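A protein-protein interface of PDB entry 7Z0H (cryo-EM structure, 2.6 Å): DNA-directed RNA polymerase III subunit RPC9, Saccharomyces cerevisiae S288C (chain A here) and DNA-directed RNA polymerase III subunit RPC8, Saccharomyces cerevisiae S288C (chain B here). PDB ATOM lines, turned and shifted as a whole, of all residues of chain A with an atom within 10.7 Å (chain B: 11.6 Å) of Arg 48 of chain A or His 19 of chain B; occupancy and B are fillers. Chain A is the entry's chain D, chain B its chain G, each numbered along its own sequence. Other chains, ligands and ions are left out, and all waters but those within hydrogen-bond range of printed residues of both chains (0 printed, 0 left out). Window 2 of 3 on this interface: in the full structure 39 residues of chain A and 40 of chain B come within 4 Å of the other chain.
Arg 48 of chain A touches just one residue of chain B: His 19 (3.7 Å).
His 19 of chain B touches just one residue of chain A: Arg 48.
No residue of chain B comes within 4 Å of Arg 41 of chain A.
No residue of chain B comes within 4 Å of Lys 43 of chain A.
Lys 45 of chain A touches none of the printed residues of chain B.
Gln 46 of chain A touches none of the printed residues of chain B.
No residue of chain B comes within 4 Å of Asn 47 of chain A.
Gln 17 of chain B touches just one residue of chain A: Pro 49 (3.9 Å).
Of the printed residues of chain A, Arg 20 of chain B touches Tyr 50 (3.7 Å).
Of the printed residues of chain B, Asn 51 of chain A touches His 28.
Of the printed residues of chain A, His 28 of chain B touches Asn 51 (3.9 Å).
Gly 64 of chain B touches none of the printed residues of chain A.
A ring nitrogen (ND1) of His 19 of chain B sits at hydrogen-bond distance from the backbone carbonyl oxygen (O) of Asp 16 of chain B, 3.0 Å away.
The backbone carbonyl oxygen (O) of Ser 24 of chain B lies within hydrogen-bond range of the guanidinium group (NH1) of Arg 20 of chain B (3.3 Å).
The side-chain amide oxygen (OD1) of Asn 32 of chain B lies close to the backbone carbonyl oxygen (O) of His 28 of chain B (2.6 Å).
Of the 21 printed residues of chain B, 4 touch a printed residue of chain A.
Hydrophobic or aromatic side chains of chain B within 4 Å of the printed part of chain A: His 19 and His 28.
Along chain B the printed residues that touch a printed residue of chain A span positions 17 to 28.
Of the 14 printed residues of chain A, 4 touch a printed residue of chain B.
Hydrophobic or aromatic side chains of chain A within 4 Å of the printed part of chain B: Tyr 50.
Among the printed residues, no Asp or Glu carboxylate lies within 4 Å of a Lys or Arg side-chain nitrogen of the other chain.
CD of Arg 48 of chain A touches NE2 of His 19 of chain B (3.7 Å).
Pro 49 of chain A touches Gln 17 of chain B (O to NE2, 3.9 Å).
NH2 of Arg 20 of chain B touches CD2 of Tyr 50 of chain A, at 3.7 Å.
CE1 of His 28 of chain B touches O of Asn 51 of chain A (3.9 Å).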
ATOM      1  N   LYS A  39     -16.440  38.560 -15.590  1.00  0.00           N
ATOM      2  CA  LYS A  39     -17.670  38.327 -16.339  1.00  0.00           C
ATOM      3  C   LYS A  39     -18.200  36.917 -16.110  1.00  0.00           C
ATOM      4  O   LYS A  39     -19.398  36.727 -15.864  1.00  0.00           O
ATOM      5  N   SER A  40     -17.324  35.916 -16.181  1.00  0.00           N
ATOM      6  CA  SER A  40     -17.743  34.526 -16.063  1.00  0.00           C
ATOM      7  C   SER A  40     -18.538  34.106 -17.292  1.00  0.00           C
ATOM      8  O   SER A  40     -18.303  34.611 -18.395  1.00  0.00           O
ATOM      9  N   ARG A  41     -19.488  33.185 -17.112  1.00  0.00           N
ATOM     10  CA  ARG A  41     -20.271  32.703 -18.244  1.00  0.00           C
ATOM     11  C   ARG A  41     -21.306  33.724 -18.696  1.00  0.00           C
ATOM     12  O   ARG A  41     -21.633  33.786 -19.887  1.00  0.00           O
ATOM     13  N   SER A  42     -21.836  34.522 -17.771  1.00  0.00           N
ATOM     14  CA  SER A  42     -22.855  35.509 -18.105  1.00  0.00           C
ATOM     15  C   SER A  42     -24.211  34.845 -18.317  1.00  0.00           C
ATOM     16  O   SER A  42     -25.219  35.531 -18.519  1.00  0.00           O
ATOM     17  N   LYS A  43     -24.246  33.511 -18.271  1.00  0.00           N
ATOM     18  CA  LYS A  43     -25.504  32.788 -18.405  1.00  0.00           C
ATOM     19  C   LYS A  43     -26.346  32.852 -17.139  1.00  0.00           C
ATOM     20  O   LYS A  43     -27.578  32.805 -17.226  1.00  0.00           O
ATOM     21  N   GLY A  44     -25.714  32.959 -15.971  1.00  0.00           N
ATOM     22  CA  GLY A  44     -26.406  33.080 -14.706  1.00  0.00           C
ATOM     23  C   GLY A  44     -25.976  32.082 -13.652  1.00  0.00           C
ATOM     24  O   GLY A  44     -26.144  32.356 -12.456  1.00  0.00           O
ATOM     25  N   LYS A  45     -25.422  30.936 -14.053  1.00  0.00           N
ATOM     26  CA  LYS A  45     -25.024  29.895 -13.112  1.00  0.00           C
ATOM     27  C   LYS A  45     -23.599  29.405 -13.346  1.00  0.00           C
ATOM     28  O   LYS A  45     -23.301  28.233 -13.095  1.00  0.00           O
ATOM     29  N   GLN A  46     -22.708  30.280 -13.810  1.00  0.00           N
ATOM     30  CA  GLN A  46     -21.342  29.879 -14.119  1.00  0.00           C
ATOM     31  C   GLN A  46     -21.144  29.791 -15.626  1.00  0.00           C
ATOM     32  O   GLN A  46     -22.066  30.085 -16.395  1.00  0.00           O
ATOM     33  N   ASN A  47     -19.948  29.395 -16.056  1.00  0.00           N
ATOM     34  CA  ASN A  47     -19.653  29.298 -17.480  1.00  0.00           C
ATOM     35  C   ASN A  47     -20.551  28.257 -18.131  1.00  0.00           C
ATOM     36  O   ASN A  47     -20.545  27.087 -17.732  1.00  0.00           O
ATOM     37  N   ARG A  48     -21.311  28.684 -19.137  1.00  0.00           N
ATOM     38  CA  ARG A  48     -22.273  27.837 -19.832  1.00  0.00           C
ATOM     39  C   ARG A  48     -23.157  27.087 -18.831  1.00  0.00           C
ATOM     40  O   ARG A  48     -23.244  25.856 -18.876  1.00  0.00           O
ATOM     41  CB  ARG A  48     -21.566  26.867 -20.771  1.00  0.00           C
ATOM     42  CG  ARG A  48     -22.462  26.203 -21.812  1.00  0.00           C
ATOM     43  CD  ARG A  48     -23.208  27.216 -22.665  1.00  0.00           C
ATOM     44  NE  ARG A  48     -22.310  27.997 -23.505  1.00  0.00           N
ATOM     45  CZ  ARG A  48     -22.706  28.941 -24.348  1.00  0.00           C
ATOM     46  NH1 ARG A  48     -23.986  29.239 -24.500  1.00  0.00           N
ATOM     47  NH2 ARG A  48     -21.796  29.596 -25.062  1.00  0.00           N
ATOM     48  N   PRO A  49     -23.883  27.821 -17.964  1.00  0.00           N
ATOM     49  CA  PRO A  49     -24.497  27.238 -16.759  1.00  0.00           C
ATOM     50  C   PRO A  49     -24.064  25.836 -16.348  1.00  0.00           C
ATOM     51  O   PRO A  49     -24.873  24.903 -16.356  1.00  0.00           O
ATOM     52  CB  PRO A  49     -25.999  27.299 -17.100  1.00  0.00           C
ATOM     53  CG  PRO A  49     -26.068  28.043 -18.488  1.00  0.00           C
ATOM     54  CD  PRO A  49     -24.794  28.831 -18.504  1.00  0.00           C
ATOM     55  N   TYR A  50     -22.789  25.678 -15.997  1.00  0.00           N
ATOM     56  CA  TYR A  50     -22.303  24.462 -15.360  1.00  0.00           C
ATOM     57  C   TYR A  50     -21.173  24.814 -14.402  1.00  0.00           C
ATOM     58  O   TYR A  50     -20.508  25.843 -14.542  1.00  0.00           O
ATOM     59  CB  TYR A  50     -21.843  23.406 -16.387  1.00  0.00           C
ATOM     60  CG  TYR A  50     -20.626  23.773 -17.218  1.00  0.00           C
ATOM     61  CD1 TYR A  50     -19.346  23.705 -16.687  1.00  0.00           C
ATOM     62  CD2 TYR A  50     -20.755  24.135 -18.550  1.00  0.00           C
ATOM     63  CE1 TYR A  50     -18.236  24.028 -17.441  1.00  0.00           C
ATOM     64  CE2 TYR A  50     -19.648  24.455 -19.316  1.00  0.00           C
ATOM     65  CZ  TYR A  50     -18.392  24.400 -18.755  1.00  0.00           C
ATOM     66  OH  TYR A  50     -17.287  24.717 -19.510  1.00  0.00           O
ATOM     67  N   ASN A  51     -20.966  23.941 -13.417  1.00  0.00           N
ATOM     68  CA  ASN A  51     -19.899  24.111 -12.442  1.00  0.00           C
ATOM     69  C   ASN A  51     -19.485  22.740 -11.927  1.00  0.00           C
ATOM     70  O   ASN A  51     -20.235  21.766 -12.030  1.00  0.00           O
ATOM     71  CB  ASN A  51     -20.330  25.020 -11.281  1.00  0.00           C
ATOM     72  CG  ASN A  51     -19.156  25.508 -10.453  1.00  0.00           C
ATOM     73  OD1 ASN A  51     -18.811  24.914  -9.431  1.00  0.00           O
ATOM     74  ND2 ASN A  51     -18.532  26.595 -10.893  1.00  0.00           N
ATOM     75  N   HIS A  52     -18.280  22.675 -11.362  1.00  0.00           N
ATOM     76  CA  HIS A  52     -17.701  21.428 -10.859  1.00  0.00           C
ATOM     77  C   HIS A  52     -17.296  21.576  -9.397  1.00  0.00           C
ATOM     78  O   HIS A  52     -16.107  21.688  -9.076  1.00  0.00           O
ATOM     79  CB  HIS A  52     -16.496  20.998 -11.696  1.00  0.00           C
ATOM     80  CG  HIS A  52     -16.572  21.400 -13.137  1.00  0.00           C
ATOM     81  ND1 HIS A  52     -17.720  21.266 -13.887  1.00  0.00           N
ATOM     82  CD2 HIS A  52     -15.645  21.943 -13.961  1.00  0.00           C
ATOM     83  CE1 HIS A  52     -17.492  21.695 -15.114  1.00  0.00           C
ATOM     84  NE2 HIS A  52     -16.243  22.117 -15.185  1.00  0.00           N
ATOM     85  N   ILE B  13     -31.820  14.851 -17.663  1.00  0.00           N
ATOM     86  CA  ILE B  13     -31.161  15.926 -18.397  1.00  0.00           C
ATOM     87  C   ILE B  13     -32.157  17.073 -18.543  1.00  0.00           C
ATOM     88  O   ILE B  13     -33.198  16.891 -19.193  1.00  0.00           O
ATOM     89  CB  ILE B  13     -30.666  15.453 -19.767  1.00  0.00           C
ATOM     90  CG1 ILE B  13     -29.547  14.422 -19.599  1.00  0.00           C
ATOM     91  CG2 ILE B  13     -30.197  16.632 -20.605  1.00  0.00           C
ATOM     92  CD1 ILE B  13     -29.055  13.851 -20.902  1.00  0.00           C
ATOM     93  N   PRO B  14     -31.890  18.240 -17.967  1.00  0.00           N
ATOM     94  CA  PRO B  14     -32.806  19.372 -18.119  1.00  0.00           C
ATOM     95  C   PRO B  14     -32.790  19.889 -19.545  1.00  0.00           C
ATOM     96  O   PRO B  14     -31.812  19.680 -20.279  1.00  0.00           O
ATOM     97  CB  PRO B  14     -32.249  20.421 -17.141  1.00  0.00           C
ATOM     98  CG  PRO B  14     -31.238  19.704 -16.304  1.00  0.00           C
ATOM     99  CD  PRO B  14     -30.729  18.575 -17.129  1.00  0.00           C
ATOM    100  N   PRO B  15     -33.858  20.560 -19.979  1.00  0.00           N
ATOM    101  CA  PRO B  15     -33.851  21.149 -21.327  1.00  0.00           C
ATOM    102  C   PRO B  15     -32.773  22.199 -21.523  1.00  0.00           C
ATOM    103  O   PRO B  15     -32.437  22.509 -22.673  1.00  0.00           O
ATOM    104  CB  PRO B  15     -35.259  21.745 -21.455  1.00  0.00           C
ATOM    105  CG  PRO B  15     -36.081  20.973 -20.475  1.00  0.00           C
ATOM    106  CD  PRO B  15     -35.164  20.722 -19.321  1.00  0.00           C
ATOM    107  N   ASP B  16     -32.223  22.760 -20.442  1.00  0.00           N
ATOM    108  CA  ASP B  16     -31.086  23.665 -20.576  1.00  0.00           C
ATOM    109  C   ASP B  16     -29.905  22.960 -21.227  1.00  0.00           C
ATOM    110  O   ASP B  16     -29.181  23.555 -22.034  1.00  0.00           O
ATOM    111  CB  ASP B  16     -30.669  24.205 -19.207  1.00  0.00           C
ATOM    112  CG  ASP B  16     -31.607  25.267 -18.682  1.00  0.00           C
ATOM    113  OD1 ASP B  16     -32.824  25.006 -18.629  1.00  0.00           O
ATOM    114  OD2 ASP B  16     -31.132  26.368 -18.334  1.00  0.00           O
ATOM    115  N   GLN B  17     -29.695  21.691 -20.885  1.00  0.00           N
ATOM    116  CA  GLN B  17     -28.525  20.934 -21.306  1.00  0.00           C
ATOM    117  C   GLN B  17     -28.801  20.044 -22.511  1.00  0.00           C
ATOM    118  O   GLN B  17     -28.066  19.079 -22.740  1.00  0.00           O
ATOM    119  CB  GLN B  17     -28.000  20.095 -20.142  1.00  0.00           C
ATOM    120  CG  GLN B  17     -27.777  20.884 -18.867  1.00  0.00           C
ATOM    121  CD  GLN B  17     -26.354  21.388 -18.742  1.00  0.00           C
ATOM    122  OE1 GLN B  17     -25.486  20.703 -18.200  1.00  0.00           O
ATOM    123  NE2 GLN B  17     -26.104  22.590 -19.247  1.00  0.00           N
ATOM    124  N   PHE B  18     -29.848  20.341 -23.282  1.00  0.00           N
ATOM    125  CA  PHE B  18     -30.096  19.576 -24.498  1.00  0.00           C
ATOM    126  C   PHE B  18     -29.101  19.916 -25.600  1.00  0.00           C
ATOM    127  O   PHE B  18     -28.902  19.105 -26.509  1.00  0.00           O
ATOM    128  CB  PHE B  18     -31.522  19.817 -24.997  1.00  0.00           C
ATOM    129  CG  PHE B  18     -32.571  19.065 -24.227  1.00  0.00           C
ATOM    130  CD1 PHE B  18     -32.219  18.048 -23.357  1.00  0.00           C
ATOM    131  CD2 PHE B  18     -33.913  19.373 -24.380  1.00  0.00           C
ATOM    132  CE1 PHE B  18     -33.183  17.358 -22.651  1.00  0.00           C
ATOM    133  CE2 PHE B  18     -34.881  18.684 -23.675  1.00  0.00           C
ATOM    134  CZ  PHE B  18     -34.516  17.677 -22.810  1.00  0.00           C
ATOM    135  N   HIS B  19     -28.470  21.093 -25.536  1.00  0.00           N
ATOM    136  CA  HIS B  19     -27.554  21.501 -26.597  1.00  0.00           C
ATOM    137  C   HIS B  19     -26.236  20.739 -26.524  1.00  0.00           C
ATOM    138  O   HIS B  19     -25.715  20.296 -27.555  1.00  0.00           O
ATOM    139  CB  HIS B  19     -27.313  23.011 -26.531  1.00  0.00           C
ATOM    140  CG  HIS B  19     -26.574  23.456 -25.308  1.00  0.00           C
ATOM    141  ND1 HIS B  19     -27.029  23.209 -24.031  1.00  0.00           N
ATOM    142  CD2 HIS B  19     -25.409  24.133 -25.167  1.00  0.00           C
ATOM    143  CE1 HIS B  19     -26.178  23.713 -23.156  1.00  0.00           C
ATOM    144  NE2 HIS B  19     -25.186  24.280 -23.820  1.00  0.00           N
ATOM    145  N   ARG B  20     -25.679  20.577 -25.326  1.00  0.00           N
ATOM    146  CA  ARG B  20     -24.437  19.833 -25.185  1.00  0.00           C
ATOM    147  C   ARG B  20     -24.664  18.371 -25.543  1.00  0.00           C
ATOM    148  O   ARG B  20     -25.762  17.832 -25.380  1.00  0.00           O
ATOM    149  CB  ARG B  20     -23.888  19.948 -23.763  1.00  0.00           C
ATOM    150  CG  ARG B  20     -24.935  19.873 -22.670  1.00  0.00           C
ATOM    151  CD  ARG B  20     -24.326  19.390 -21.363  1.00  0.00           C
ATOM    152  NE  ARG B  20     -23.222  20.236 -20.925  1.00  0.00           N
ATOM    153  CZ  ARG B  20     -22.263  19.849 -20.093  1.00  0.00           C
ATOM    154  NH1 ARG B  20     -22.237  18.626 -19.590  1.00  0.00           N
ATOM    155  NH2 ARG B  20     -21.307  20.711 -19.758  1.00  0.00           N
ATOM    156  N   ASP B  21     -23.614  17.733 -26.055  1.00  0.00           N
ATOM    157  CA  ASP B  21     -23.730  16.344 -26.476  1.00  0.00           C
ATOM    158  C   ASP B  21     -24.179  15.468 -25.311  1.00  0.00           C
ATOM    159  O   ASP B  21     -23.757  15.651 -24.163  1.00  0.00           O
ATOM    160  CB  ASP B  21     -22.407  15.849 -27.068  1.00  0.00           C
ATOM    161  CG  ASP B  21     -21.410  15.429 -26.014  1.00  0.00           C
ATOM    162  OD1 ASP B  21     -20.825  16.325 -25.375  1.00  0.00           O
ATOM    163  OD2 ASP B  21     -21.213  14.212 -25.823  1.00  0.00           O
ATOM    164  N   THR B  22     -25.077  14.529 -25.619  1.00  0.00           N
ATOM    165  CA  THR B  22     -25.773  13.792 -24.573  1.00  0.00           C
ATOM    166  C   THR B  22     -24.816  12.949 -23.742  1.00  0.00           C
ATOM    167  O   THR B  22     -25.078  12.711 -22.560  1.00  0.00           O
ATOM    168  CB  THR B  22     -26.867  12.915 -25.185  1.00  0.00           C
ATOM    169  OG1 THR B  22     -27.579  13.665 -26.177  1.00  0.00           O
ATOM    170  CG2 THR B  22     -27.846  12.460 -24.116  1.00  0.00           C
ATOM    171  N   ILE B  23     -23.703  12.505 -24.327  1.00  0.00           N
ATOM    172  CA  ILE B  23     -22.701  11.782 -23.547  1.00  0.00           C
ATOM    173  C   ILE B  23     -22.187  12.657 -22.411  1.00  0.00           C
ATOM    174  O   ILE B  23     -22.161  12.244 -21.244  1.00  0.00           O
ATOM    175  CB  ILE B  23     -21.552  11.305 -24.454  1.00  0.00           C
ATOM    176  CG1 ILE B  23     -22.021  10.166 -25.363  1.00  0.00           C
ATOM    177  CG2 ILE B  23     -20.344  10.896 -23.619  1.00  0.00           C
ATOM    178  CD1 ILE B  23     -21.738   8.781 -24.821  1.00  0.00           C
ATOM    179  N   SER B  24     -21.798  13.893 -22.734  1.00  0.00           N
ATOM    180  CA  SER B  24     -21.298  14.797 -21.705  1.00  0.00           C
ATOM    181  C   SER B  24     -22.399  15.195 -20.734  1.00  0.00           C
ATOM    182  O   SER B  24     -22.144  15.346 -19.538  1.00  0.00           O
ATOM    183  CB  SER B  24     -20.676  16.039 -22.340  1.00  0.00           C
ATOM    184  OG  SER B  24     -21.640  17.064 -22.507  1.00  0.00           O
ATOM    185  N   ALA B  25     -23.628  15.374 -21.226  1.00  0.00           N
ATOM    186  CA  ALA B  25     -24.728  15.723 -20.328  1.00  0.00           C
ATOM    187  C   ALA B  25     -24.981  14.616 -19.309  1.00  0.00           C
ATOM    188  O   ALA B  25     -25.121  14.877 -18.106  1.00  0.00           O
ATOM    189  CB  ALA B  25     -25.991  16.014 -21.137  1.00  0.00           C
ATOM    190  N   ILE B  26     -25.030  13.366 -19.775  1.00  0.00           N
ATOM    191  CA  ILE B  26     -25.252  12.233 -18.886  1.00  0.00           C
ATOM    192  C   ILE B  26     -24.095  12.082 -17.911  1.00  0.00           C
ATOM    193  O   ILE B  26     -24.302  11.831 -16.719  1.00  0.00           O
ATOM    194  CB  ILE B  26     -25.469  10.947 -19.707  1.00  0.00           C
ATOM    195  CG1 ILE B  26     -26.774  11.025 -20.497  1.00  0.00           C
ATOM    196  CG2 ILE B  26     -25.481   9.728 -18.802  1.00  0.00           C
ATOM    197  CD1 ILE B  26     -26.936   9.908 -21.501  1.00  0.00           C
ATOM    198  N   HIS B  28     -22.099  14.428 -16.863  1.00  0.00           N
ATOM    199  CA  HIS B  28     -22.179  15.536 -15.920  1.00  0.00           C
ATOM    200  C   HIS B  28     -23.216  15.262 -14.838  1.00  0.00           C
ATOM    201  O   HIS B  28     -22.954  15.465 -13.648  1.00  0.00           O
ATOM    202  CB  HIS B  28     -22.498  16.825 -16.681  1.00  0.00           C
ATOM    203  CG  HIS B  28     -22.835  17.990 -15.803  1.00  0.00           C
ATOM    204  ND1 HIS B  28     -21.880  18.855 -15.316  1.00  0.00           N
ATOM    205  CD2 HIS B  28     -24.025  18.449 -15.347  1.00  0.00           C
ATOM    206  CE1 HIS B  28     -22.465  19.789 -14.586  1.00  0.00           C
ATOM    207  NE2 HIS B  28     -23.766  19.564 -14.588  1.00  0.00           N
ATOM    208  N   GLN B  29     -24.401  14.783 -15.233  1.00  0.00           N
ATOM    209  CA  GLN B  29     -25.424  14.452 -14.241  1.00  0.00           C
ATOM    210  C   GLN B  29     -24.952  13.340 -13.311  1.00  0.00           C
ATOM    211  O   GLN B  29     -25.141  13.413 -12.087  1.00  0.00           O
ATOM    212  CB  GLN B  29     -26.723  14.048 -14.939  1.00  0.00           C
ATOM    213  CG  GLN B  29     -27.363  15.154 -15.757  1.00  0.00           C
ATOM    214  CD  GLN B  29     -27.744  16.350 -14.913  1.00  0.00           C
ATOM    215  OE1 GLN B  29     -28.377  16.208 -13.868  1.00  0.00           O
ATOM    216  NE2 GLN B  29     -27.359  17.537 -15.361  1.00  0.00           N
ATOM    217  N   ASN B  32     -22.550  14.903 -10.824  1.00  0.00           N
ATOM    218  CA  ASN B  32     -23.244  15.627  -9.763  1.00  0.00           C
ATOM    219  C   ASN B  32     -23.991  14.692  -8.823  1.00  0.00           C
ATOM    220  O   ASN B  32     -24.316  15.092  -7.701  1.00  0.00           O
ATOM    221  CB  ASN B  32     -24.217  16.673 -10.322  1.00  0.00           C
ATOM    222  CG  ASN B  32     -23.547  17.676 -11.241  1.00  0.00           C
ATOM    223  OD1 ASN B  32     -23.694  17.620 -12.457  1.00  0.00           O
ATOM    224  ND2 ASN B  32     -22.795  18.602 -10.656  1.00  0.00           N
ATOM    225  N   GLY B  64     -40.780  17.803 -18.866  1.00  0.00           N
ATOM    226  CA  GLY B  64     -40.099  18.267 -20.051  1.00  0.00           C
ATOM    227  C   GLY B  64     -38.639  17.877 -20.129  1.00  0.00           C
ATOM    228  O   GLY B  64     -38.058  17.911 -21.219  1.00  0.00           O
ATOM    229  N   SER B  65     -38.032  17.506 -19.005  1.00  0.00           N
ATOM    230  CA  SER B  65     -36.666  17.010 -19.009  1.00  0.00           C
ATOM    231  C   SER B  65     -36.619  15.596 -19.580  1.00  0.00           C
ATOM    232  O   SER B  65     -37.617  14.873 -19.608  1.00  0.00           O
ATOM    233  CB  SER B  65     -36.088  17.024 -17.596  1.00  0.00           C
ATOM    234  OG  SER B  65     -36.555  18.143 -16.865  1.00  0.00           O
ATOM    235  N   SER B  66     -35.435  15.208 -20.045  1.00  0.00           N
ATOM    236  CA  SER B  66     -35.215  13.873 -20.581  1.00  0.00           C
ATOM    237  C   SER B  66     -34.687  12.970 -19.474  1.00  0.00           C
ATOM    238  O   SER B  66     -33.626  13.236 -18.902  1.00  0.00           O
ATOM    239  CB  SER B  66     -34.237  13.918 -21.754  1.00  0.00           C
ATOM    240  OG  SER B  66     -34.282  12.717 -22.501  1.00  0.00           O
ATOM    241  N   ILE B  68     -33.162   9.448 -18.668  1.00  0.00           N
ATOM    242  CA  ILE B  68     -32.415   8.449 -19.421  1.00  0.00           C
ATOM    243  C   ILE B  68     -32.018   7.323 -18.480  1.00  0.00           C
ATOM    244  O   ILE B  68     -31.359   7.563 -17.461  1.00  0.00           O
ATOM    245  CB  ILE B  68     -31.175   9.057 -20.092  1.00  0.00           C
ATOM    246  CG1 ILE B  68     -31.578  10.222 -20.999  1.00  0.00           C
ATOM    247  CG2 ILE B  68     -30.418   7.995 -20.863  1.00  0.00           C
ATOM    248  CD1 ILE B  68     -30.485  10.677 -21.928  1.00  0.00           C
